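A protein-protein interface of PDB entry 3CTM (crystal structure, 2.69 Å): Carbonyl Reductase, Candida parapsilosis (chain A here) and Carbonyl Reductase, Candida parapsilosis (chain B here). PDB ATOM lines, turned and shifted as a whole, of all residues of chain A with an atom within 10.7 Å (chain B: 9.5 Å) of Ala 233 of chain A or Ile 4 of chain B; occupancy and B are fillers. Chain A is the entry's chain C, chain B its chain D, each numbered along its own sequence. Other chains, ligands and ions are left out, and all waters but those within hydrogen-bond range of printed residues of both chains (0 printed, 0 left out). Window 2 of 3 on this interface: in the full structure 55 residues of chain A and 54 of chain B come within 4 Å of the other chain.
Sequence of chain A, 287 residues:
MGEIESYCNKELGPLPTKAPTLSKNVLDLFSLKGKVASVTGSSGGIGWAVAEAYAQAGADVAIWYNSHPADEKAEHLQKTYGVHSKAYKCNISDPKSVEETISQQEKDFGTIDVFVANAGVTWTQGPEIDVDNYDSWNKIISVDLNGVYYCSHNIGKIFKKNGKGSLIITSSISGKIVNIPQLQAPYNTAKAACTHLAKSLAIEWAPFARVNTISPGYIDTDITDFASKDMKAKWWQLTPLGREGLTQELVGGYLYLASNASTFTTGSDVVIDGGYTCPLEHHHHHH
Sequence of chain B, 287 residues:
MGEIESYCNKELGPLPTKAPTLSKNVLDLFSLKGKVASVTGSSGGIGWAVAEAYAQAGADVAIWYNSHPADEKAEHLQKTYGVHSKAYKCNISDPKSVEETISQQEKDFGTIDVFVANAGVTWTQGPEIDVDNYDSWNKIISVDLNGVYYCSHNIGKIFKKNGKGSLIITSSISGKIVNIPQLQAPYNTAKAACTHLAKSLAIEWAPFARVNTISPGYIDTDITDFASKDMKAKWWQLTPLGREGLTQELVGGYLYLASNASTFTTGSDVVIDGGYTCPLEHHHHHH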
ATOM      1  N   TYR A 218      13.798  -4.251 -22.253  1.00  0.00           N
ATOM      2  CA  TYR A 218      12.364  -4.022 -22.044  1.00  0.00           C
ATOM      3  C   TYR A 218      11.992  -4.410 -20.612  1.00  0.00           C
ATOM      4  O   TYR A 218      12.016  -5.596 -20.254  1.00  0.00           O
ATOM      5  CB  TYR A 218      11.545  -4.811 -23.066  1.00  0.00           C
ATOM      6  CG  TYR A 218      11.740  -4.322 -24.481  1.00  0.00           C
ATOM      7  CD1 TYR A 218      11.084  -3.171 -24.940  1.00  0.00           C
ATOM      8  CD2 TYR A 218      12.601  -4.985 -25.351  1.00  0.00           C
ATOM      9  CE1 TYR A 218      11.276  -2.707 -26.232  1.00  0.00           C
ATOM     10  CE2 TYR A 218      12.793  -4.536 -26.644  1.00  0.00           C
ATOM     11  CZ  TYR A 218      12.137  -3.400 -27.077  1.00  0.00           C
ATOM     12  OH  TYR A 218      12.338  -2.959 -28.361  1.00  0.00           O
ATOM     13  N   ASP A 220       9.191  -4.078 -17.363  1.00  0.00           N
ATOM     14  CA  ASP A 220       7.796  -3.771 -17.033  1.00  0.00           C
ATOM     15  C   ASP A 220       7.670  -2.587 -16.080  1.00  0.00           C
ATOM     16  O   ASP A 220       7.573  -2.756 -14.866  1.00  0.00           O
ATOM     17  CB  ASP A 220       7.092  -4.993 -16.439  1.00  0.00           C
ATOM     18  CG  ASP A 220       5.587  -4.981 -16.703  1.00  0.00           C
ATOM     19  OD1 ASP A 220       5.177  -4.426 -17.749  1.00  0.00           O
ATOM     20  OD2 ASP A 220       4.817  -5.534 -15.885  1.00  0.00           O
ATOM     21  N   THR A 224       7.928   1.627 -20.682  1.00  0.00           N
ATOM     22  CA  THR A 224       7.288   0.862 -21.741  1.00  0.00           C
ATOM     23  C   THR A 224       5.819   0.562 -21.454  1.00  0.00           C
ATOM     24  O   THR A 224       5.100   0.140 -22.364  1.00  0.00           O
ATOM     25  CB  THR A 224       8.050  -0.449 -21.991  1.00  0.00           C
ATOM     26  OG1 THR A 224       7.859  -1.344 -20.881  1.00  0.00           O
ATOM     27  CG2 THR A 224       9.545  -0.183 -22.201  1.00  0.00           C
ATOM     28  N   ALA A 227       2.705   0.678 -23.985  1.00  0.00           N
ATOM     29  CA  ALA A 227       2.475  -0.193 -25.116  1.00  0.00           C
ATOM     30  C   ALA A 227       1.332  -1.147 -24.826  1.00  0.00           C
ATOM     31  O   ALA A 227       0.897  -1.310 -23.687  1.00  0.00           O
ATOM     32  CB  ALA A 227       3.739  -0.974 -25.459  1.00  0.00           C
ATOM     33  N   SER A 228       0.843  -1.784 -25.883  1.00  0.00           N
ATOM     34  CA  SER A 228      -0.242  -2.740 -25.762  1.00  0.00           C
ATOM     35  C   SER A 228       0.323  -4.135 -25.557  1.00  0.00           C
ATOM     36  O   SER A 228       1.496  -4.401 -25.830  1.00  0.00           O
ATOM     37  CB  SER A 228      -1.131  -2.722 -27.005  1.00  0.00           C
ATOM     38  OG  SER A 228      -0.616  -3.580 -28.010  1.00  0.00           O
ATOM     39  N   LYS A 229      -0.543  -5.040 -25.093  1.00  0.00           N
ATOM     40  CA  LYS A 229      -0.133  -6.427 -24.920  1.00  0.00           C
ATOM     41  C   LYS A 229       0.291  -7.062 -26.240  1.00  0.00           C
ATOM     42  O   LYS A 229       1.029  -8.049 -26.224  1.00  0.00           O
ATOM     43  CB  LYS A 229      -1.263  -7.232 -24.257  1.00  0.00           C
ATOM     44  CG  LYS A 229      -1.366  -7.094 -22.702  1.00  0.00           C
ATOM     45  CD  LYS A 229      -0.022  -6.714 -22.025  1.00  0.00           C
ATOM     46  CE  LYS A 229      -0.162  -6.386 -20.527  1.00  0.00           C
ATOM     47  NZ  LYS A 229      -0.742  -5.022 -20.273  1.00  0.00           N
ATOM     48  N   ASP A 230      -0.132  -6.503 -27.379  1.00  0.00           N
ATOM     49  CA  ASP A 230       0.242  -7.049 -28.682  1.00  0.00           C
ATOM     50  C   ASP A 230       1.641  -6.612 -29.095  1.00  0.00           C
ATOM     51  O   ASP A 230       2.364  -7.386 -29.738  1.00  0.00           O
ATOM     52  CB  ASP A 230      -0.773  -6.626 -29.750  1.00  0.00           C
ATOM     53  CG  ASP A 230      -2.145  -7.282 -29.565  1.00  0.00           C
ATOM     54  OD1 ASP A 230      -2.348  -7.994 -28.551  1.00  0.00           O
ATOM     55  OD2 ASP A 230      -3.026  -7.090 -30.436  1.00  0.00           O
ATOM     56  N   MET A 231       2.031  -5.378 -28.740  1.00  0.00           N
ATOM     57  CA  MET A 231       3.392  -4.911 -28.997  1.00  0.00           C
ATOM     58  C   MET A 231       4.380  -5.568 -28.039  1.00  0.00           C
ATOM     59  O   MET A 231       5.454  -6.029 -28.451  1.00  0.00           O
ATOM     60  CB  MET A 231       3.481  -3.388 -28.858  1.00  0.00           C
ATOM     61  CG  MET A 231       2.751  -2.558 -29.906  1.00  0.00           C
ATOM     62  SD  MET A 231       2.280  -0.933 -29.259  1.00  0.00           S
ATOM     63  CE  MET A 231       3.925  -0.257 -28.933  1.00  0.00           C
ATOM     64  N   LYS A 232       4.034  -5.599 -26.746  1.00  0.00           N
ATOM     65  CA  LYS A 232       4.844  -6.291 -25.749  1.00  0.00           C
ATOM     66  C   LYS A 232       5.121  -7.731 -26.154  1.00  0.00           C
ATOM     67  O   LYS A 232       6.210  -8.257 -25.889  1.00  0.00           O
ATOM     68  CB  LYS A 232       4.147  -6.237 -24.393  1.00  0.00           C
ATOM     69  CG  LYS A 232       4.415  -4.967 -23.621  1.00  0.00           C
ATOM     70  CD  LYS A 232       3.579  -4.895 -22.360  1.00  0.00           C
ATOM     71  CE  LYS A 232       4.021  -3.743 -21.442  1.00  0.00           C
ATOM     72  NZ  LYS A 232       4.930  -4.199 -20.324  1.00  0.00           N
ATOM     73  N   ALA A 233       4.162  -8.375 -26.829  1.00  0.00           N
ATOM     74  CA  ALA A 233       4.370  -9.738 -27.314  1.00  0.00           C
ATOM     75  C   ALA A 233       5.531  -9.811 -28.303  1.00  0.00           C
ATOM     76  O   ALA A 233       6.268 -10.804 -28.334  1.00  0.00           O
ATOM     77  CB  ALA A 233       3.085 -10.266 -27.949  1.00  0.00           C
ATOM     78  N   LYS A 234       5.711  -8.771 -29.119  1.00  0.00           N
ATOM     79  CA  LYS A 234       6.843  -8.756 -30.049  1.00  0.00           C
ATOM     80  C   LYS A 234       8.172  -8.744 -29.299  1.00  0.00           C
ATOM     81  O   LYS A 234       9.175  -9.272 -29.793  1.00  0.00           O
ATOM     82  CB  LYS A 234       6.723  -7.553 -30.998  1.00  0.00           C
ATOM     83  CG  LYS A 234       5.266  -7.263 -31.389  1.00  0.00           C
ATOM     84  CD  LYS A 234       5.105  -6.227 -32.492  1.00  0.00           C
ATOM     85  CE  LYS A 234       3.613  -5.949 -32.733  1.00  0.00           C
ATOM     86  NZ  LYS A 234       3.340  -4.926 -33.794  1.00  0.00           N
ATOM     87  N   TRP A 235       8.183  -8.176 -28.093  1.00  0.00           N
ATOM     88  CA  TRP A 235       9.385  -8.194 -27.275  1.00  0.00           C
ATOM     89  C   TRP A 235       9.680  -9.602 -26.776  1.00  0.00           C
ATOM     90  O   TRP A 235      10.775 -10.130 -27.004  1.00  0.00           O
ATOM     91  CB  TRP A 235       9.229  -7.219 -26.109  1.00  0.00           C
ATOM     92  CG  TRP A 235       8.862  -5.832 -26.559  1.00  0.00           C
ATOM     93  CD1 TRP A 235       8.977  -5.337 -27.807  1.00  0.00           C
ATOM     94  CD2 TRP A 235       8.298  -4.779 -25.762  1.00  0.00           C
ATOM     95  NE1 TRP A 235       8.543  -4.041 -27.853  1.00  0.00           N
ATOM     96  CE2 TRP A 235       8.111  -3.675 -26.609  1.00  0.00           C
ATOM     97  CE3 TRP A 235       7.947  -4.661 -24.418  1.00  0.00           C
ATOM     98  CZ2 TRP A 235       7.594  -2.470 -26.162  1.00  0.00           C
ATOM     99  CZ3 TRP A 235       7.437  -3.471 -23.976  1.00  0.00           C
ATOM    100  CH2 TRP A 235       7.260  -2.388 -24.845  1.00  0.00           C
ATOM    101  N   TRP A 236       8.705 -10.237 -26.112  1.00  0.00           N
ATOM    102  CA  TRP A 236       8.952 -11.547 -25.517  1.00  0.00           C
ATOM    103  C   TRP A 236       9.473 -12.540 -26.545  1.00  0.00           C
ATOM    104  O   TRP A 236      10.205 -13.480 -26.203  1.00  0.00           O
ATOM    105  CB  TRP A 236       7.682 -12.088 -24.855  1.00  0.00           C
ATOM    106  CG  TRP A 236       6.936 -11.082 -24.022  1.00  0.00           C
ATOM    107  CD1 TRP A 236       7.463 -10.027 -23.310  1.00  0.00           C
ATOM    108  CD2 TRP A 236       5.525 -11.032 -23.815  1.00  0.00           C
ATOM    109  NE1 TRP A 236       6.456  -9.330 -22.677  1.00  0.00           N
ATOM    110  CE2 TRP A 236       5.259  -9.922 -22.977  1.00  0.00           C
ATOM    111  CE3 TRP A 236       4.456 -11.815 -24.260  1.00  0.00           C
ATOM    112  CZ2 TRP A 236       3.971  -9.587 -22.575  1.00  0.00           C
ATOM    113  CZ3 TRP A 236       3.181 -11.481 -23.864  1.00  0.00           C
ATOM    114  CH2 TRP A 236       2.945 -10.378 -23.025  1.00  0.00           C
ATOM    115  N   GLN A 237       9.135 -12.335 -27.809  1.00  0.00           N
ATOM    116  CA  GLN A 237       9.546 -13.274 -28.840  1.00  0.00           C
ATOM    117  C   GLN A 237      10.990 -13.075 -29.244  1.00  0.00           C
ATOM    118  O   GLN A 237      11.641 -14.022 -29.696  1.00  0.00           O
ATOM    119  CB  GLN A 237       8.647 -13.124 -30.056  1.00  0.00           C
ATOM    120  CG  GLN A 237       7.279 -13.639 -29.798  1.00  0.00           C
ATOM    121  CD  GLN A 237       6.358 -13.331 -30.915  1.00  0.00           C
ATOM    122  OE1 GLN A 237       5.909 -12.204 -31.062  1.00  0.00           O
ATOM    123  NE2 GLN A 237       6.094 -14.323 -31.748  1.00  0.00           N
ATOM    124  N   LEU A 238      11.491 -11.854 -29.098  1.00  0.00           N
ATOM    125  CA  LEU A 238      12.855 -11.526 -29.473  1.00  0.00           C
ATOM    126  C   LEU A 238      13.830 -11.610 -28.307  1.00  0.00           C
ATOM    127  O   LEU A 238      15.034 -11.752 -28.548  1.00  0.00           O
ATOM    128  CB  LEU A 238      12.887 -10.128 -30.100  1.00  0.00           C
ATOM    129  CG  LEU A 238      12.098 -10.089 -31.408  1.00  0.00           C
ATOM    130  CD1 LEU A 238      11.920  -8.671 -31.904  1.00  0.00           C
ATOM    131  CD2 LEU A 238      12.816 -10.920 -32.449  1.00  0.00           C
ATOM    132  N   THR A 239      13.332 -11.548 -27.057  1.00  0.00           N
ATOM    133  CA  THR A 239      14.134 -11.649 -25.844  1.00  0.00           C
ATOM    134  C   THR A 239      14.466 -13.102 -25.520  1.00  0.00           C
ATOM    135  O   THR A 239      13.569 -13.888 -25.187  1.00  0.00           O
ATOM    136  CB  THR A 239      13.402 -11.023 -24.659  1.00  0.00           C
ATOM    137  OG1 THR A 239      12.895  -9.734 -25.012  1.00  0.00           O
ATOM    138  CG2 THR A 239      14.334 -10.882 -23.488  1.00  0.00           C
ATOM    139  N   PRO A 240      15.741 -13.487 -25.597  1.00  0.00           N
ATOM    140  CA  PRO A 240      16.135 -14.866 -25.262  1.00  0.00           C
ATOM    141  C   PRO A 240      15.610 -15.393 -23.940  1.00  0.00           C
ATOM    142  O   PRO A 240      15.389 -16.596 -23.829  1.00  0.00           O
ATOM    143  CB  PRO A 240      17.664 -14.776 -25.247  1.00  0.00           C
ATOM    144  CG  PRO A 240      17.951 -13.743 -26.259  1.00  0.00           C
ATOM    145  CD  PRO A 240      16.871 -12.714 -26.131  1.00  0.00           C
ATOM    146  N   LEU A 241      15.413 -14.561 -22.924  1.00  0.00           N
ATOM    147  CA  LEU A 241      14.867 -15.094 -21.685  1.00  0.00           C
ATOM    148  C   LEU A 241      13.367 -15.276 -21.762  1.00  0.00           C
ATOM    149  O   LEU A 241      12.788 -15.909 -20.875  1.00  0.00           O
ATOM    150  CB  LEU A 241      15.226 -14.199 -20.499  1.00  0.00           C
ATOM    151  CG  LEU A 241      16.685 -14.262 -20.027  1.00  0.00           C
ATOM    152  CD1 LEU A 241      16.887 -13.315 -18.817  1.00  0.00           C
ATOM    153  CD2 LEU A 241      17.183 -15.723 -19.742  1.00  0.00           C
ATOM    154  N   GLY A 242      12.740 -14.737 -22.801  1.00  0.00           N
ATOM    155  CA  GLY A 242      11.348 -14.969 -23.064  1.00  0.00           C
ATOM    156  C   GLY A 242      10.391 -14.049 -22.355  1.00  0.00           C
ATOM    157  O   GLY A 242       9.191 -14.346 -22.328  1.00  0.00           O
ATOM    158  N   ARG A 243      10.863 -12.937 -21.793  1.00  0.00           N
ATOM    159  CA  ARG A 243      10.001 -12.093 -20.968  1.00  0.00           C
ATOM    160  C   ARG A 243      10.540 -10.674 -20.951  1.00  0.00           C
ATOM    161  O   ARG A 243      11.583 -10.375 -21.530  1.00  0.00           O
ATOM    162  CB  ARG A 243       9.895 -12.625 -19.537  1.00  0.00           C
ATOM    163  CG  ARG A 243      11.224 -12.945 -18.908  1.00  0.00           C
ATOM    164  CD  ARG A 243      11.077 -13.307 -17.440  1.00  0.00           C
ATOM    165  NE  ARG A 243      12.367 -13.565 -16.808  1.00  0.00           N
ATOM    166  CZ  ARG A 243      13.059 -12.670 -16.112  1.00  0.00           C
ATOM    167  NH1 ARG A 243      12.613 -11.437 -15.929  1.00  0.00           N
ATOM    168  NH2 ARG A 243      14.233 -13.020 -15.589  1.00  0.00           N
ATOM    169  N   GLU A 244       9.798  -9.799 -20.292  1.00  0.00           N
ATOM    170  CA  GLU A 244      10.275  -8.489 -19.898  1.00  0.00           C
ATOM    171  C   GLU A 244      11.016  -8.586 -18.569  1.00  0.00           C
ATOM    172  O   GLU A 244      10.824  -9.523 -17.784  1.00  0.00           O
ATOM    173  CB  GLU A 244       9.112  -7.514 -19.743  1.00  0.00           C
ATOM    174  CG  GLU A 244       8.746  -6.748 -20.967  1.00  0.00           C
ATOM    175  CD  GLU A 244       7.399  -6.080 -20.836  1.00  0.00           C
ATOM    176  OE1 GLU A 244       6.361  -6.788 -20.894  1.00  0.00           O
ATOM    177  OE2 GLU A 244       7.388  -4.841 -20.656  1.00  0.00           O
ATOM    178  N   TYR A 276      18.534  -9.439 -25.219  1.00  0.00           N
ATOM    179  CA  TYR A 276      17.956  -8.903 -26.440  1.00  0.00           C
ATOM    180  C   TYR A 276      19.013  -8.374 -27.394  1.00  0.00           C
ATOM    181  O   TYR A 276      18.784  -8.380 -28.606  1.00  0.00           O
ATOM    182  CB  TYR A 276      16.952  -7.810 -26.112  1.00  0.00           C
ATOM    183  CG  TYR A 276      16.019  -7.424 -27.258  1.00  0.00           C
ATOM    184  CD1 TYR A 276      16.493  -6.740 -28.374  1.00  0.00           C
ATOM    185  CD2 TYR A 276      14.649  -7.682 -27.189  1.00  0.00           C
ATOM    186  CE1 TYR A 276      15.657  -6.367 -29.394  1.00  0.00           C
ATOM    187  CE2 TYR A 276      13.802  -7.305 -28.215  1.00  0.00           C
ATOM    188  CZ  TYR A 276      14.318  -6.647 -29.315  1.00  0.00           C
ATOM    189  OH  TYR A 276      13.498  -6.256 -30.346  1.00  0.00           O
ATOM    190  N   GLU B   3      -1.249 -18.264 -29.118  1.00  0.00           N
ATOM    191  CA  GLU B   3      -0.226 -18.505 -28.113  1.00  0.00           C
ATOM    192  C   GLU B   3       1.151 -18.116 -28.652  1.00  0.00           C
ATOM    193  O   GLU B   3       1.612 -18.636 -29.676  1.00  0.00           O
ATOM    194  CB  GLU B   3      -0.230 -19.963 -27.672  1.00  0.00           C
ATOM    195  CG  GLU B   3       1.097 -20.422 -27.096  1.00  0.00           C
ATOM    196  CD  GLU B   3       1.514 -21.793 -27.601  1.00  0.00           C
ATOM    197  OE1 GLU B   3       1.106 -22.809 -26.992  1.00  0.00           O
ATOM    198  OE2 GLU B   3       2.254 -21.855 -28.608  1.00  0.00           O
ATOM    199  N   ILE B   4       1.811 -17.213 -27.930  1.00  0.00           N
ATOM    200  CA  ILE B   4       2.966 -16.477 -28.443  1.00  0.00           C
ATOM    201  C   ILE B   4       4.197 -17.375 -28.332  1.00  0.00           C
ATOM    202  O   ILE B   4       4.756 -17.550 -27.250  1.00  0.00           O
ATOM    203  CB  ILE B   4       3.154 -15.152 -27.700  1.00  0.00           C
ATOM    204  CG1 ILE B   4       1.837 -14.363 -27.679  1.00  0.00           C
ATOM    205  CG2 ILE B   4       4.248 -14.326 -28.335  1.00  0.00           C
ATOM    206  CD1 ILE B   4       1.530 -13.638 -28.987  1.00  0.00           C
ATOM    207  N   GLU B   5       4.621 -17.949 -29.458  1.00  0.00           N
ATOM    208  CA  GLU B   5       5.841 -18.741 -29.526  1.00  0.00           C
ATOM    209  C   GLU B   5       7.063 -17.830 -29.670  1.00  0.00           C
ATOM    210  O   GLU B   5       6.974 -16.694 -30.143  1.00  0.00           O
ATOM    211  CB  GLU B   5       5.769 -19.724 -30.697  1.00  0.00           C
ATOM    212  CG  GLU B   5       6.714 -20.940 -30.625  1.00  0.00           C
ATOM    213  CD  GLU B   5       6.178 -22.106 -29.778  1.00  0.00           C
ATOM    214  OE1 GLU B   5       6.199 -22.022 -28.528  1.00  0.00           O
ATOM    215  OE2 GLU B   5       5.728 -23.112 -30.375  1.00  0.00           O
ATOM    216  N   SER B   6       8.213 -18.344 -29.251  1.00  0.00           N
ATOM    217  CA  SER B   6       9.452 -17.577 -29.230  1.00  0.00           C
ATOM    218  C   SER B   6      10.168 -17.648 -30.580  1.00  0.00           C
ATOM    219  O   SER B   6       9.969 -18.576 -31.369  1.00  0.00           O
ATOM    220  CB  SER B   6      10.364 -18.082 -28.099  1.00  0.00           C
ATOM    221  OG  SER B   6      11.745 -17.926 -28.392  1.00  0.00           O
ATOM    222  N   TYR B   7      11.008 -16.647 -30.840  1.00  0.00           N
ATOM    223  CA  TYR B   7      11.789 -16.604 -32.079  1.00  0.00           C
ATOM    224  C   TYR B   7      13.284 -16.863 -31.862  1.00  0.00           C
ATOM    225  O   TYR B   7      14.046 -16.871 -32.830  1.00  0.00           O
ATOM    226  CB  TYR B   7      11.641 -15.244 -32.784  1.00  0.00           C
ATOM    227  CG  TYR B   7      10.283 -14.956 -33.393  1.00  0.00           C
ATOM    228  CD1 TYR B   7       9.374 -15.982 -33.654  1.00  0.00           C
ATOM    229  CD2 TYR B   7       9.897 -13.645 -33.681  1.00  0.00           C
ATOM    230  CE1 TYR B   7       8.129 -15.712 -34.201  1.00  0.00           C
ATOM    231  CE2 TYR B   7       8.653 -13.365 -34.223  1.00  0.00           C
ATOM    232  CZ  TYR B   7       7.774 -14.401 -34.479  1.00  0.00           C
ATOM    233  OH  TYR B   7       6.536 -14.130 -35.021  1.00  0.00           O
ATOM    234  N   ASN B   9      14.441 -19.205 -29.282  1.00  0.00           N
ATOM    235  CA  ASN B   9      14.499 -20.584 -28.861  1.00  0.00           C
ATOM    236  C   ASN B   9      13.144 -21.030 -28.326  1.00  0.00           C
ATOM    237  O   ASN B   9      12.541 -20.364 -27.473  1.00  0.00           O
ATOM    238  CB  ASN B   9      15.587 -20.762 -27.816  1.00  0.00           C
ATOM    239  CG  ASN B   9      15.493 -22.072 -27.105  1.00  0.00           C
ATOM    240  OD1 ASN B   9      14.948 -23.052 -27.620  1.00  0.00           O
ATOM    241  ND2 ASN B   9      16.036 -22.109 -25.910  1.00  0.00           N
ATOM    242  N   LYS B  10      12.682 -22.178 -28.834  1.00  0.00           N
ATOM    243  CA  LYS B  10      11.304 -22.607 -28.638  1.00  0.00           C
ATOM    244  C   LYS B  10      11.107 -23.425 -27.371  1.00  0.00           C
ATOM    245  O   LYS B  10       9.958 -23.665 -26.982  1.00  0.00           O
ATOM    246  CB  LYS B  10      10.818 -23.393 -29.863  1.00  0.00           C
ATOM    247  CG  LYS B  10      10.035 -22.523 -30.859  1.00  0.00           C
ATOM    248  CD  LYS B  10      10.202 -22.984 -32.307  1.00  0.00           C
ATOM    249  CE  LYS B  10       9.130 -22.371 -33.210  1.00  0.00           C
ATOM    250  NZ  LYS B  10       8.582 -23.323 -34.235  1.00  0.00           N
ATOM    251  N   LEU B  12      11.473 -22.257 -24.622  1.00  0.00           N
ATOM    252  CA  LEU B  12      10.879 -21.334 -23.671  1.00  0.00           C
ATOM    253  C   LEU B  12       9.393 -21.612 -23.445  1.00  0.00           C
ATOM    254  O   LEU B  12       8.852 -21.213 -22.407  1.00  0.00           O
ATOM    255  CB  LEU B  12      11.095 -19.900 -24.155  1.00  0.00           C
ATOM    256  CG  LEU B  12      12.560 -19.503 -24.300  1.00  0.00           C
ATOM    257  CD1 LEU B  12      12.665 -18.201 -25.084  1.00  0.00           C
ATOM    258  CD2 LEU B  12      13.221 -19.404 -22.923  1.00  0.00           C
ATOM    259  N   GLY B  13       8.723 -22.289 -24.380  1.00  0.00           N
ATOM    260  CA  GLY B  13       7.321 -22.601 -24.237  1.00  0.00           C
ATOM    261  C   GLY B  13       6.468 -21.363 -24.397  1.00  0.00           C
ATOM    262  O   GLY B  13       6.937 -20.325 -24.868  1.00  0.00           O
ATOM    263  N   PRO B  14       5.194 -21.449 -24.021  1.00  0.00           N
ATOM    264  CA  PRO B  14       4.311 -20.278 -24.142  1.00  0.00           C
ATOM    265  C   PRO B  14       4.859 -19.084 -23.371  1.00  0.00           C
ATOM    266  O   PRO B  14       5.266 -19.197 -22.211  1.00  0.00           O
ATOM    267  CB  PRO B  14       2.971 -20.771 -23.575  1.00  0.00           C
ATOM    268  CG  PRO B  14       3.277 -22.053 -22.868  1.00  0.00           C
ATOM    269  CD  PRO B  14       4.472 -22.645 -23.564  1.00  0.00           C
ATOM    270  N   LEU B  15       4.889 -17.964 -24.025  1.00  0.00           N
ATOM    271  CA  LEU B  15       5.486 -16.717 -23.587  1.00  0.00           C
ATOM    272  C   LEU B  15       4.436 -15.804 -22.963  1.00  0.00           C
ATOM    273  O   LEU B  15       3.256 -15.865 -23.320  1.00  0.00           O
ATOM    274  CB  LEU B  15       6.154 -16.011 -24.767  1.00  0.00           C
ATOM    275  CG  LEU B  15       7.385 -16.701 -25.351  1.00  0.00           C
ATOM    276  CD1 LEU B  15       7.955 -15.867 -26.474  1.00  0.00           C
ATOM    277  CD2 LEU B  15       8.422 -16.928 -24.279  1.00  0.00           C
ATOM    278  N   PRO B  16       4.823 -14.946 -22.011  1.00  0.00           N
ATOM    279  CA  PRO B  16       6.206 -14.784 -21.556  1.00  0.00           C
ATOM    280  C   PRO B  16       6.606 -15.799 -20.492  1.00  0.00           C
ATOM    281  O   PRO B  16       5.756 -16.151 -19.662  1.00  0.00           O
ATOM    282  CB  PRO B  16       6.217 -13.365 -20.972  1.00  0.00           C
ATOM    283  CG  PRO B  16       4.757 -13.033 -20.658  1.00  0.00           C
ATOM    284  CD  PRO B  16       3.882 -14.110 -21.244  1.00  0.00           C
ATOM    285  N   THR B  17       7.867 -16.246 -20.520  1.00  0.00           N
ATOM    286  CA  THR B  17       8.425 -16.999 -19.404  1.00  0.00           C
ATOM    287  C   THR B  17       8.229 -16.228 -18.111  1.00  0.00           C
ATOM    288  O   THR B  17       8.073 -15.007 -18.120  1.00  0.00           O
ATOM    289  CB  THR B  17       9.912 -17.289 -19.597  1.00  0.00           C
ATOM    290  OG1 THR B  17      10.638 -16.057 -19.549  1.00  0.00           O
ATOM    291  CG2 THR B  17      10.174 -18.017 -20.912  1.00  0.00           C
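The backbone carbonyl oxygen of Leu 241 of chain A is in hydrogen-bond range of the side-chain hydroxyl of Thr 17 of chain B (2.5 Å). The backbone NH (N) of Tyr 7 of chain B lies within hydrogen-bond range of the backbone carbonyl oxygen (O) of Gln 237 of chain A (2.9 Å). The backbone NH (N) of Thr 17 of chain B sits at hydrogen-bond distance from the backbone carbonyl oxygen (O) of Gly 242 of chain A, at 2.9 Å. O of Glu 5 of chain B lies within hydrogen-bond range of NE2 of Gln 237 of chain A.
Thr 224 of chain A touches none of the printed residues of chain B. Trp 236 of chain A touches two residues of chain B. Of the printed residues of chain B, Pro 240 of chain A touches Leu 12 (3.4 Å). Printed residues of chain B within 4 Å of Leu 241 of chain A: Thr 17 (2.5 Å). Of the printed residues of chain B, Arg 243 of chain A touches Pro 16 and Thr 17. Tyr 276 of chain A touches none of the printed residues of chain B. Ile 4 of chain B touches two residues of chain A. Of chain A, only Gln 237 (3.0 Å) comes within 4 Å of Glu 5 of chain B. No residue of chain A comes within 4 Å of Pro 14 of chain B. The nearest residue of chain B that does not touch Ala 233 of chain A is Leu 15 of chain B (5.7 Å). The nearest residue of chain A that does not touch Ile 4 of chain B is Trp 236 of chain A (4.8 Å). The nearest printed residue of chain A that does not touch Thr 17 of chain B is Glu 244 of chain A (5.9 Å).
Hydrophobic or aromatic side chains of chain B within 4 Å of the printed part of chain A: Ile 4, Tyr 7, Leu 12, Leu 15 and Pro 16. Among the printed residues, 14 pairs touch across the chains. Among the printed residues, no Asp or Glu carboxylate lies within 4 Å of a Lys or Arg side-chain nitrogen of the other chain.
Among the printed residues, pairs that only touch across the chains: Ala 233 of chain A with Ile 4 of chain B (3.9 Å), Trp 236 of chain A with Leu 15 of chain B (3.3 Å), Trp 236 of chain A with Pro 16 of chain B (3.7 Å), Gln 237 of chain A with Ile 4 of chain B (3.4 Å), Gln 237 of chain A with Leu 15 of chain B (3.9 Å), Pro 240 of chain A with Leu 12 of chain B (3.4 Å), Gly 242 of chain A with Leu 15 of chain B (3.3 Å), Gly 242 of chain A with Pro 16 of chain B (3.1 Å), Arg 243 of chain A with Pro 16 of chain B (3.99 Å) and Arg 243 of chain A with Thr 17 of chain B (3.2 Å).
The side-chain carboxylate of Glu 244 of chain A sits at hydrogen-bond distance from the indole nitrogen of Trp 236 of chain A, 3.1 Å away. O of Ile 4 of chain B sits close to N of Leu 15 of chain B (3.3 Å). The backbone carbonyl oxygen (O) of Lys 232 of chain A lies close to the indole nitrogen (NE1) of Trp 236 of chain A (3.4 Å). O of Ala 233 of chain A lies close to OE1 of Gln 237 of chain A, at 3.1 Å.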
